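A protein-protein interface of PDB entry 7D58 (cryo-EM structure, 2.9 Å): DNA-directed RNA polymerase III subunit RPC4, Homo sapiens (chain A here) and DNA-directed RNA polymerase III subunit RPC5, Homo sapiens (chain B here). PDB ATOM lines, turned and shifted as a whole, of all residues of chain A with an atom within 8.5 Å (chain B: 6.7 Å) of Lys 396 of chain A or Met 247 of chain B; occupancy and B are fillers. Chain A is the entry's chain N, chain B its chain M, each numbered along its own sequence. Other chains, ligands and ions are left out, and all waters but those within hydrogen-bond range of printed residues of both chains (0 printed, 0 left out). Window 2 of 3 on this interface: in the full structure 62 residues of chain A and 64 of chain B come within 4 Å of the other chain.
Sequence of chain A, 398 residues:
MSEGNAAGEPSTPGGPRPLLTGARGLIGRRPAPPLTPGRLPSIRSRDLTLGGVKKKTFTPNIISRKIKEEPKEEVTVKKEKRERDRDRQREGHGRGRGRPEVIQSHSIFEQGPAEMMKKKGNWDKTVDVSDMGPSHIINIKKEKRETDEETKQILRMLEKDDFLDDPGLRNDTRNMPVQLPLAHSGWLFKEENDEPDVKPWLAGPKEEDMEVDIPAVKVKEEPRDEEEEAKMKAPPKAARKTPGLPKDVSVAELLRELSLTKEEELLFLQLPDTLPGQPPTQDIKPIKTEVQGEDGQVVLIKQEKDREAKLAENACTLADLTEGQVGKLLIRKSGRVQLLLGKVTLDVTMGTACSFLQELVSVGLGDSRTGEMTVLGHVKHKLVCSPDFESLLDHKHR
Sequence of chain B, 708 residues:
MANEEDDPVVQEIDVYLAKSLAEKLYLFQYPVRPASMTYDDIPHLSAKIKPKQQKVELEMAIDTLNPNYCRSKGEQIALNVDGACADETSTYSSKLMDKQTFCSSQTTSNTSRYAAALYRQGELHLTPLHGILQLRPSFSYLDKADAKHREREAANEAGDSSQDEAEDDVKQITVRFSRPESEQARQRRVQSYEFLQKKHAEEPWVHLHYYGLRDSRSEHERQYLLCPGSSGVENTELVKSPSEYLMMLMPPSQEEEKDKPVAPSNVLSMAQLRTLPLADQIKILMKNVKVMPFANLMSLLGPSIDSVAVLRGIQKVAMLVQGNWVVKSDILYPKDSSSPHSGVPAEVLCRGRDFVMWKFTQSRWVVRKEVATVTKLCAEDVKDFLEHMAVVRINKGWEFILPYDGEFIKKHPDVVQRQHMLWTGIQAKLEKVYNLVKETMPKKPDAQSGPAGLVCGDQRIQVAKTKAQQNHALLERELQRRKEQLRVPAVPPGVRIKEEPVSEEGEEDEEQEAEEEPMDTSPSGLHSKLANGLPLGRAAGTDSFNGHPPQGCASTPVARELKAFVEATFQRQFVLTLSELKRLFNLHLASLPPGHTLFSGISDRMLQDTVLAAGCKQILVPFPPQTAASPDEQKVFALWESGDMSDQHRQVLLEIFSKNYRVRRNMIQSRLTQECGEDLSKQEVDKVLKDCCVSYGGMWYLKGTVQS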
ATOM      1  N   PHE A 389      17.300  15.299  -3.539  1.00  0.00           N
ATOM      2  CA  PHE A 389      16.874  14.325  -4.533  1.00  0.00           C
ATOM      3  C   PHE A 389      16.827  14.902  -5.942  1.00  0.00           C
ATOM      4  O   PHE A 389      16.719  14.135  -6.906  1.00  0.00           O
ATOM      5  CB  PHE A 389      15.502  13.755  -4.153  1.00  0.00           C
ATOM      6  CG  PHE A 389      15.465  13.131  -2.784  1.00  0.00           C
ATOM      7  CD1 PHE A 389      15.842  11.810  -2.600  1.00  0.00           C
ATOM      8  CD2 PHE A 389      15.062  13.866  -1.682  1.00  0.00           C
ATOM      9  CE1 PHE A 389      15.812  11.234  -1.342  1.00  0.00           C
ATOM     10  CE2 PHE A 389      15.030  13.297  -0.421  1.00  0.00           C
ATOM     11  CZ  PHE A 389      15.407  11.979  -0.252  1.00  0.00           C
ATOM     12  N   GLU A 390      16.919  16.226  -6.086  1.00  0.00           N
ATOM     13  CA  GLU A 390      16.924  16.830  -7.415  1.00  0.00           C
ATOM     14  C   GLU A 390      18.132  16.373  -8.221  1.00  0.00           C
ATOM     15  O   GLU A 390      17.993  15.916  -9.359  1.00  0.00           O
ATOM     16  CB  GLU A 390      16.898  18.356  -7.302  1.00  0.00           C
ATOM     17  CG  GLU A 390      15.557  18.926  -6.867  1.00  0.00           C
ATOM     18  CD  GLU A 390      15.394  18.944  -5.361  1.00  0.00           C
ATOM     19  OE1 GLU A 390      16.376  18.635  -4.654  1.00  0.00           O
ATOM     20  OE2 GLU A 390      14.284  19.261  -4.883  1.00  0.00           O
ATOM     21  N   SER A 391      19.329  16.475  -7.638  1.00  0.00           N
ATOM     22  CA  SER A 391      20.533  16.058  -8.348  1.00  0.00           C
ATOM     23  C   SER A 391      20.568  14.547  -8.555  1.00  0.00           C
ATOM     24  O   SER A 391      21.051  14.072  -9.589  1.00  0.00           O
ATOM     25  CB  SER A 391      21.781  16.522  -7.596  1.00  0.00           C
ATOM     26  OG  SER A 391      21.915  15.856  -6.352  1.00  0.00           O
ATOM     27  N   LEU A 392      20.051  13.778  -7.592  1.00  0.00           N
ATOM     28  CA  LEU A 392      19.993  12.328  -7.751  1.00  0.00           C
ATOM     29  C   LEU A 392      19.110  11.945  -8.934  1.00  0.00           C
ATOM     30  O   LEU A 392      19.490  11.116  -9.771  1.00  0.00           O
ATOM     31  CB  LEU A 392      19.483  11.681  -6.461  1.00  0.00           C
ATOM     32  CG  LEU A 392      20.529  11.311  -5.403  1.00  0.00           C
ATOM     33  CD1 LEU A 392      21.074  12.549  -4.701  1.00  0.00           C
ATOM     34  CD2 LEU A 392      19.947  10.336  -4.392  1.00  0.00           C
ATOM     35  N   LEU A 393      17.924  12.554  -9.025  1.00  0.00           N
ATOM     36  CA  LEU A 393      17.040  12.288 -10.154  1.00  0.00           C
ATOM     37  C   LEU A 393      17.625  12.801 -11.463  1.00  0.00           C
ATOM     38  O   LEU A 393      17.432  12.175 -12.510  1.00  0.00           O
ATOM     39  CB  LEU A 393      15.665  12.911  -9.905  1.00  0.00           C
ATOM     40  CG  LEU A 393      14.802  12.257  -8.825  1.00  0.00           C
ATOM     41  CD1 LEU A 393      13.803  13.256  -8.266  1.00  0.00           C
ATOM     42  CD2 LEU A 393      14.087  11.036  -9.381  1.00  0.00           C
ATOM     43  N   ASP A 394      18.341  13.927 -11.429  1.00  0.00           N
ATOM     44  CA  ASP A 394      18.964  14.450 -12.642  1.00  0.00           C
ATOM     45  C   ASP A 394      20.047  13.506 -13.151  1.00  0.00           C
ATOM     46  O   ASP A 394      20.207  13.318 -14.362  1.00  0.00           O
ATOM     47  CB  ASP A 394      19.543  15.839 -12.373  1.00  0.00           C
ATOM     48  CG  ASP A 394      18.478  16.916 -12.327  1.00  0.00           C
ATOM     49  OD1 ASP A 394      18.838  18.109 -12.241  1.00  0.00           O
ATOM     50  OD2 ASP A 394      17.280  16.569 -12.380  1.00  0.00           O
ATOM     51  N   HIS A 395      20.808  12.910 -12.231  1.00  0.00           N
ATOM     52  CA  HIS A 395      21.853  11.975 -12.631  1.00  0.00           C
ATOM     53  C   HIS A 395      21.261  10.657 -13.116  1.00  0.00           C
ATOM     54  O   HIS A 395      21.742  10.075 -14.095  1.00  0.00           O
ATOM     55  CB  HIS A 395      22.816  11.735 -11.468  1.00  0.00           C
ATOM     56  CG  HIS A 395      23.765  10.600 -11.691  1.00  0.00           C
ATOM     57  ND1 HIS A 395      24.754  10.633 -12.651  1.00  0.00           N
ATOM     58  CD2 HIS A 395      23.875   9.396 -11.082  1.00  0.00           C
ATOM     59  CE1 HIS A 395      25.434   9.501 -12.620  1.00  0.00           C
ATOM     60  NE2 HIS A 395      24.920   8.732 -11.677  1.00  0.00           N
ATOM     61  N   LYS A 396      20.216  10.169 -12.443  1.00  0.00           N
ATOM     62  CA  LYS A 396      19.627   8.889 -12.821  1.00  0.00           C
ATOM     63  C   LYS A 396      18.888   8.995 -14.152  1.00  0.00           C
ATOM     64  O   LYS A 396      18.924   8.071 -14.974  1.00  0.00           O
ATOM     65  CB  LYS A 396      18.693   8.396 -11.716  1.00  0.00           C
ATOM     66  CG  LYS A 396      18.243   6.957 -11.892  1.00  0.00           C
ATOM     67  CD  LYS A 396      17.348   6.509 -10.751  1.00  0.00           C
ATOM     68  CE  LYS A 396      16.836   5.098 -10.985  1.00  0.00           C
ATOM     69  NZ  LYS A 396      15.889   4.660  -9.925  1.00  0.00           N
ATOM     70  N   HIS A 397      18.207  10.121 -14.380  1.00  0.00           N
ATOM     71  CA  HIS A 397      17.482  10.315 -15.631  1.00  0.00           C
ATOM     72  C   HIS A 397      18.440  10.394 -16.813  1.00  0.00           C
ATOM     73  O   HIS A 397      18.255   9.713 -17.827  1.00  0.00           O
ATOM     74  CB  HIS A 397      16.622  11.579 -15.541  1.00  0.00           C
ATOM     75  CG  HIS A 397      15.628  11.720 -16.653  1.00  0.00           C
ATOM     76  ND1 HIS A 397      14.306  12.038 -16.430  1.00  0.00           N
ATOM     77  CD2 HIS A 397      15.763  11.591 -17.995  1.00  0.00           C
ATOM     78  CE1 HIS A 397      13.668  12.096 -17.586  1.00  0.00           C
ATOM     79  NE2 HIS A 397      14.530  11.829 -18.551  1.00  0.00           N
ATOM     80  N   ARG A 398      19.471  11.225 -16.698  1.00  0.00           N
ATOM     81  CA  ARG A 398      20.462  11.373 -17.757  1.00  0.00           C
ATOM     82  C   ARG A 398      21.283  10.097 -17.913  1.00  0.00           C
ATOM     83  O   ARG A 398      21.135   9.368 -18.893  1.00  0.00           O
ATOM     84  CB  ARG A 398      21.377  12.567 -17.471  1.00  0.00           C
ATOM     85  CG  ARG A 398      22.360  12.895 -18.587  1.00  0.00           C
ATOM     86  CD  ARG A 398      23.753  12.367 -18.275  1.00  0.00           C
ATOM     87  NE  ARG A 398      24.250  12.863 -16.995  1.00  0.00           N
ATOM     88  CZ  ARG A 398      25.239  12.300 -16.308  1.00  0.00           C
ATOM     89  NH1 ARG A 398      25.841  11.216 -16.777  1.00  0.00           N
ATOM     90  NH2 ARG A 398      25.625  12.819 -15.151  1.00  0.00           N
ATOM     91  N   PRO B 242      25.190   8.125  -6.633  1.00  0.00           N
ATOM     92  CA  PRO B 242      23.785   8.445  -6.339  1.00  0.00           C
ATOM     93  C   PRO B 242      22.799   7.471  -6.956  1.00  0.00           C
ATOM     94  O   PRO B 242      21.720   7.264  -6.387  1.00  0.00           O
ATOM     95  CB  PRO B 242      23.616   9.861  -6.908  1.00  0.00           C
ATOM     96  CG  PRO B 242      24.745  10.034  -7.865  1.00  0.00           C
ATOM     97  CD  PRO B 242      25.879   9.241  -7.301  1.00  0.00           C
ATOM     98  N   SER B 243      23.136   6.857  -8.093  1.00  0.00           N
ATOM     99  CA  SER B 243      22.269   5.848  -8.690  1.00  0.00           C
ATOM    100  C   SER B 243      22.112   4.618  -7.807  1.00  0.00           C
ATOM    101  O   SER B 243      21.145   3.868  -7.975  1.00  0.00           O
ATOM    102  CB  SER B 243      22.807   5.433 -10.060  1.00  0.00           C
ATOM    103  OG  SER B 243      22.780   6.522 -10.965  1.00  0.00           O
ATOM    104  N   GLU B 244      23.040   4.395  -6.879  1.00  0.00           N
ATOM    105  CA  GLU B 244      22.929   3.310  -5.913  1.00  0.00           C
ATOM    106  C   GLU B 244      22.331   3.772  -4.591  1.00  0.00           C
ATOM    107  O   GLU B 244      21.549   3.034  -3.979  1.00  0.00           O
ATOM    108  CB  GLU B 244      24.306   2.681  -5.681  1.00  0.00           C
ATOM    109  CG  GLU B 244      24.856   1.958  -6.906  1.00  0.00           C
ATOM    110  CD  GLU B 244      26.263   1.428  -6.703  1.00  0.00           C
ATOM    111  OE1 GLU B 244      26.875   1.743  -5.662  1.00  0.00           O
ATOM    112  OE2 GLU B 244      26.758   0.697  -7.587  1.00  0.00           O
ATOM    113  N   TYR B 245      22.665   4.987  -4.149  1.00  0.00           N
ATOM    114  CA  TYR B 245      22.112   5.502  -2.901  1.00  0.00           C
ATOM    115  C   TYR B 245      20.614   5.762  -3.012  1.00  0.00           C
ATOM    116  O   TYR B 245      19.872   5.504  -2.058  1.00  0.00           O
ATOM    117  CB  TYR B 245      22.848   6.777  -2.490  1.00  0.00           C
ATOM    118  CG  TYR B 245      22.341   7.402  -1.210  1.00  0.00           C
ATOM    119  CD1 TYR B 245      22.246   6.659  -0.041  1.00  0.00           C
ATOM    120  CD2 TYR B 245      21.963   8.738  -1.170  1.00  0.00           C
ATOM    121  CE1 TYR B 245      21.784   7.227   1.131  1.00  0.00           C
ATOM    122  CE2 TYR B 245      21.501   9.315  -0.002  1.00  0.00           C
ATOM    123  CZ  TYR B 245      21.414   8.555   1.145  1.00  0.00           C
ATOM    124  OH  TYR B 245      20.953   9.126   2.309  1.00  0.00           O
ATOM    125  N   LEU B 246      20.150   6.260  -4.163  1.00  0.00           N
ATOM    126  CA  LEU B 246      18.718   6.474  -4.345  1.00  0.00           C
ATOM    127  C   LEU B 246      17.957   5.157  -4.393  1.00  0.00           C
ATOM    128  O   LEU B 246      16.833   5.073  -3.883  1.00  0.00           O
ATOM    129  CB  LEU B 246      18.462   7.279  -5.619  1.00  0.00           C
ATOM    130  CG  LEU B 246      17.015   7.718  -5.858  1.00  0.00           C
ATOM    131  CD1 LEU B 246      16.531   8.606  -4.721  1.00  0.00           C
ATOM    132  CD2 LEU B 246      16.876   8.430  -7.196  1.00  0.00           C
ATOM    133  N   MET B 247      18.546   4.124  -4.995  1.00  0.00           N
ATOM    134  CA  MET B 247      17.928   2.805  -4.998  1.00  0.00           C
ATOM    135  C   MET B 247      17.912   2.172  -3.614  1.00  0.00           C
ATOM    136  O   MET B 247      16.949   1.477  -3.275  1.00  0.00           O
ATOM    137  CB  MET B 247      18.654   1.885  -5.981  1.00  0.00           C
ATOM    138  CG  MET B 247      17.993   0.530  -6.177  1.00  0.00           C
ATOM    139  SD  MET B 247      16.354   0.666  -6.915  1.00  0.00           S
ATOM    140  CE  MET B 247      16.777   1.120  -8.596  1.00  0.00           C
ATOM    141  N   MET B 248      18.952   2.401  -2.809  1.00  0.00           N
ATOM    142  CA  MET B 248      18.962   1.882  -1.446  1.00  0.00           C
ATOM    143  C   MET B 248      17.963   2.619  -0.561  1.00  0.00           C
ATOM    144  O   MET B 248      17.336   2.009   0.313  1.00  0.00           O
ATOM    145  CB  MET B 248      20.372   1.977  -0.861  1.00  0.00           C
ATOM    146  CG  MET B 248      20.464   1.617   0.615  1.00  0.00           C
ATOM    147  SD  MET B 248      22.125   1.825   1.283  1.00  0.00           S
ATOM    148  CE  MET B 248      23.039   0.654   0.284  1.00  0.00           C
ATOM    149  N   LEU B 249      17.793   3.927  -0.776  1.00  0.00           N
ATOM    150  CA  LEU B 249      16.875   4.703   0.052  1.00  0.00           C
ATOM    151  C   LEU B 249      15.429   4.280  -0.174  1.00  0.00           C
ATOM    152  O   LEU B 249      14.710   3.955   0.779  1.00  0.00           O
ATOM    153  CB  LEU B 249      17.046   6.196  -0.231  1.00  0.00           C
ATOM    154  CG  LEU B 249      18.138   6.934   0.547  1.00  0.00           C
ATOM    155  CD1 LEU B 249      18.037   8.431   0.301  1.00  0.00           C
ATOM    156  CD2 LEU B 249      18.049   6.622   2.032  1.00  0.00           C
ATOM    157  N   MET B 250      14.981   4.282  -1.429  1.00  0.00           N
ATOM    158  CA  MET B 250      13.602   3.938  -1.765  1.00  0.00           C
ATOM    159  C   MET B 250      13.539   2.507  -2.283  1.00  0.00           C
ATOM    160  O   MET B 250      13.928   2.246  -3.432  1.00  0.00           O
ATOM    161  CB  MET B 250      13.044   4.911  -2.808  1.00  0.00           C
ATOM    162  CG  MET B 250      12.944   6.349  -2.323  1.00  0.00           C
ATOM    163  SD  MET B 250      11.672   6.576  -1.066  1.00  0.00           S
ATOM    164  CE  MET B 250      10.200   6.151  -1.992  1.00  0.00           C
ATOM    165  N   PRO B 251      13.067   1.552  -1.488  1.00  0.00           N
ATOM    166  CA  PRO B 251      12.999   0.163  -1.953  1.00  0.00           C
ATOM    167  C   PRO B 251      11.869  -0.025  -2.948  1.00  0.00           C
ATOM    168  O   PRO B 251      10.729   0.392  -2.694  1.00  0.00           O
ATOM    169  CB  PRO B 251      12.745  -0.627  -0.661  1.00  0.00           C
ATOM    170  CG  PRO B 251      12.048   0.339   0.232  1.00  0.00           C
ATOM    171  CD  PRO B 251      12.600   1.699  -0.099  1.00  0.00           C
ATOM    172  N   PRO B 252      12.148  -0.639  -4.100  1.00  0.00           N
ATOM    173  CA  PRO B 252      11.066  -0.897  -5.068  1.00  0.00           C
ATOM    174  C   PRO B 252       9.999  -1.842  -4.540  1.00  0.00           C
ATOM    175  O   PRO B 252       8.843  -1.782  -4.981  1.00  0.00           O
ATOM    176  CB  PRO B 252      11.815  -1.485  -6.273  1.00  0.00           C
ATOM    177  CG  PRO B 252      13.233  -1.034  -6.111  1.00  0.00           C
ATOM    178  CD  PRO B 252      13.471  -1.002  -4.634  1.00  0.00           C
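OG of Ser 243 of chain B lies close to NE2 of His 395 of chain A, at 3.2 Å.
The guanidinium group of Arg 398 of chain A is in hydrogen-bond range of a ring nitrogen (ND1) of His 395 of chain A, 3.4 Å away.
Hydrophobic or aromatic side chains of chain B within 4 Å of the printed part of chain A: Pro 242, Leu 246, Met 247 and Leu 249. Among the printed residues, 7 pairs touch across the chains. Among the printed residues, no Asp or Glu carboxylate lies within 4 Å of a Lys or Arg side-chain nitrogen of the other chain.
Among the printed residues, merely in contact across the chains: His 395 of chain A with Pro 242 of chain B (3.4 Å), Leu 392 of chain A with Leu 246 of chain B (3.6 Å), Leu 392 of chain A with Pro 242 of chain B (3.7 Å), Lys 396 of chain A with Met 247 of chain B (3.9 Å), Phe 389 of chain A with Leu 246 of chain B (3.9 Å) and Phe 389 of chain A with Leu 249 of chain B (3.9 Å).
Asp 394 of chain A touches none of the printed residues of chain B. Of the printed residues of chain B, His 395 of chain A touches Pro 242 (3.4 Å) and Ser 243 (3.1 Å). Lys 396 of chain A touches one residue of chain B. Printed residues of chain A within 4 Å of Pro 242 of chain B: Leu 392 and His 395. Tyr 245 of chain B touches none of the printed residues of chain A. Of the printed residues of chain A, Leu 246 of chain B touches Phe 389 (3.9 Å) and Leu 392 (3.6 Å). Of the printed residues of chain A, Met 247 of chain B touches Lys 396. Of the printed residues of chain A, Leu 249 of chain B touches Phe 389. The nearest residue of chain B that does not touch Lys 396 of chain A is Leu 246 of chain B (4.1 Å).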
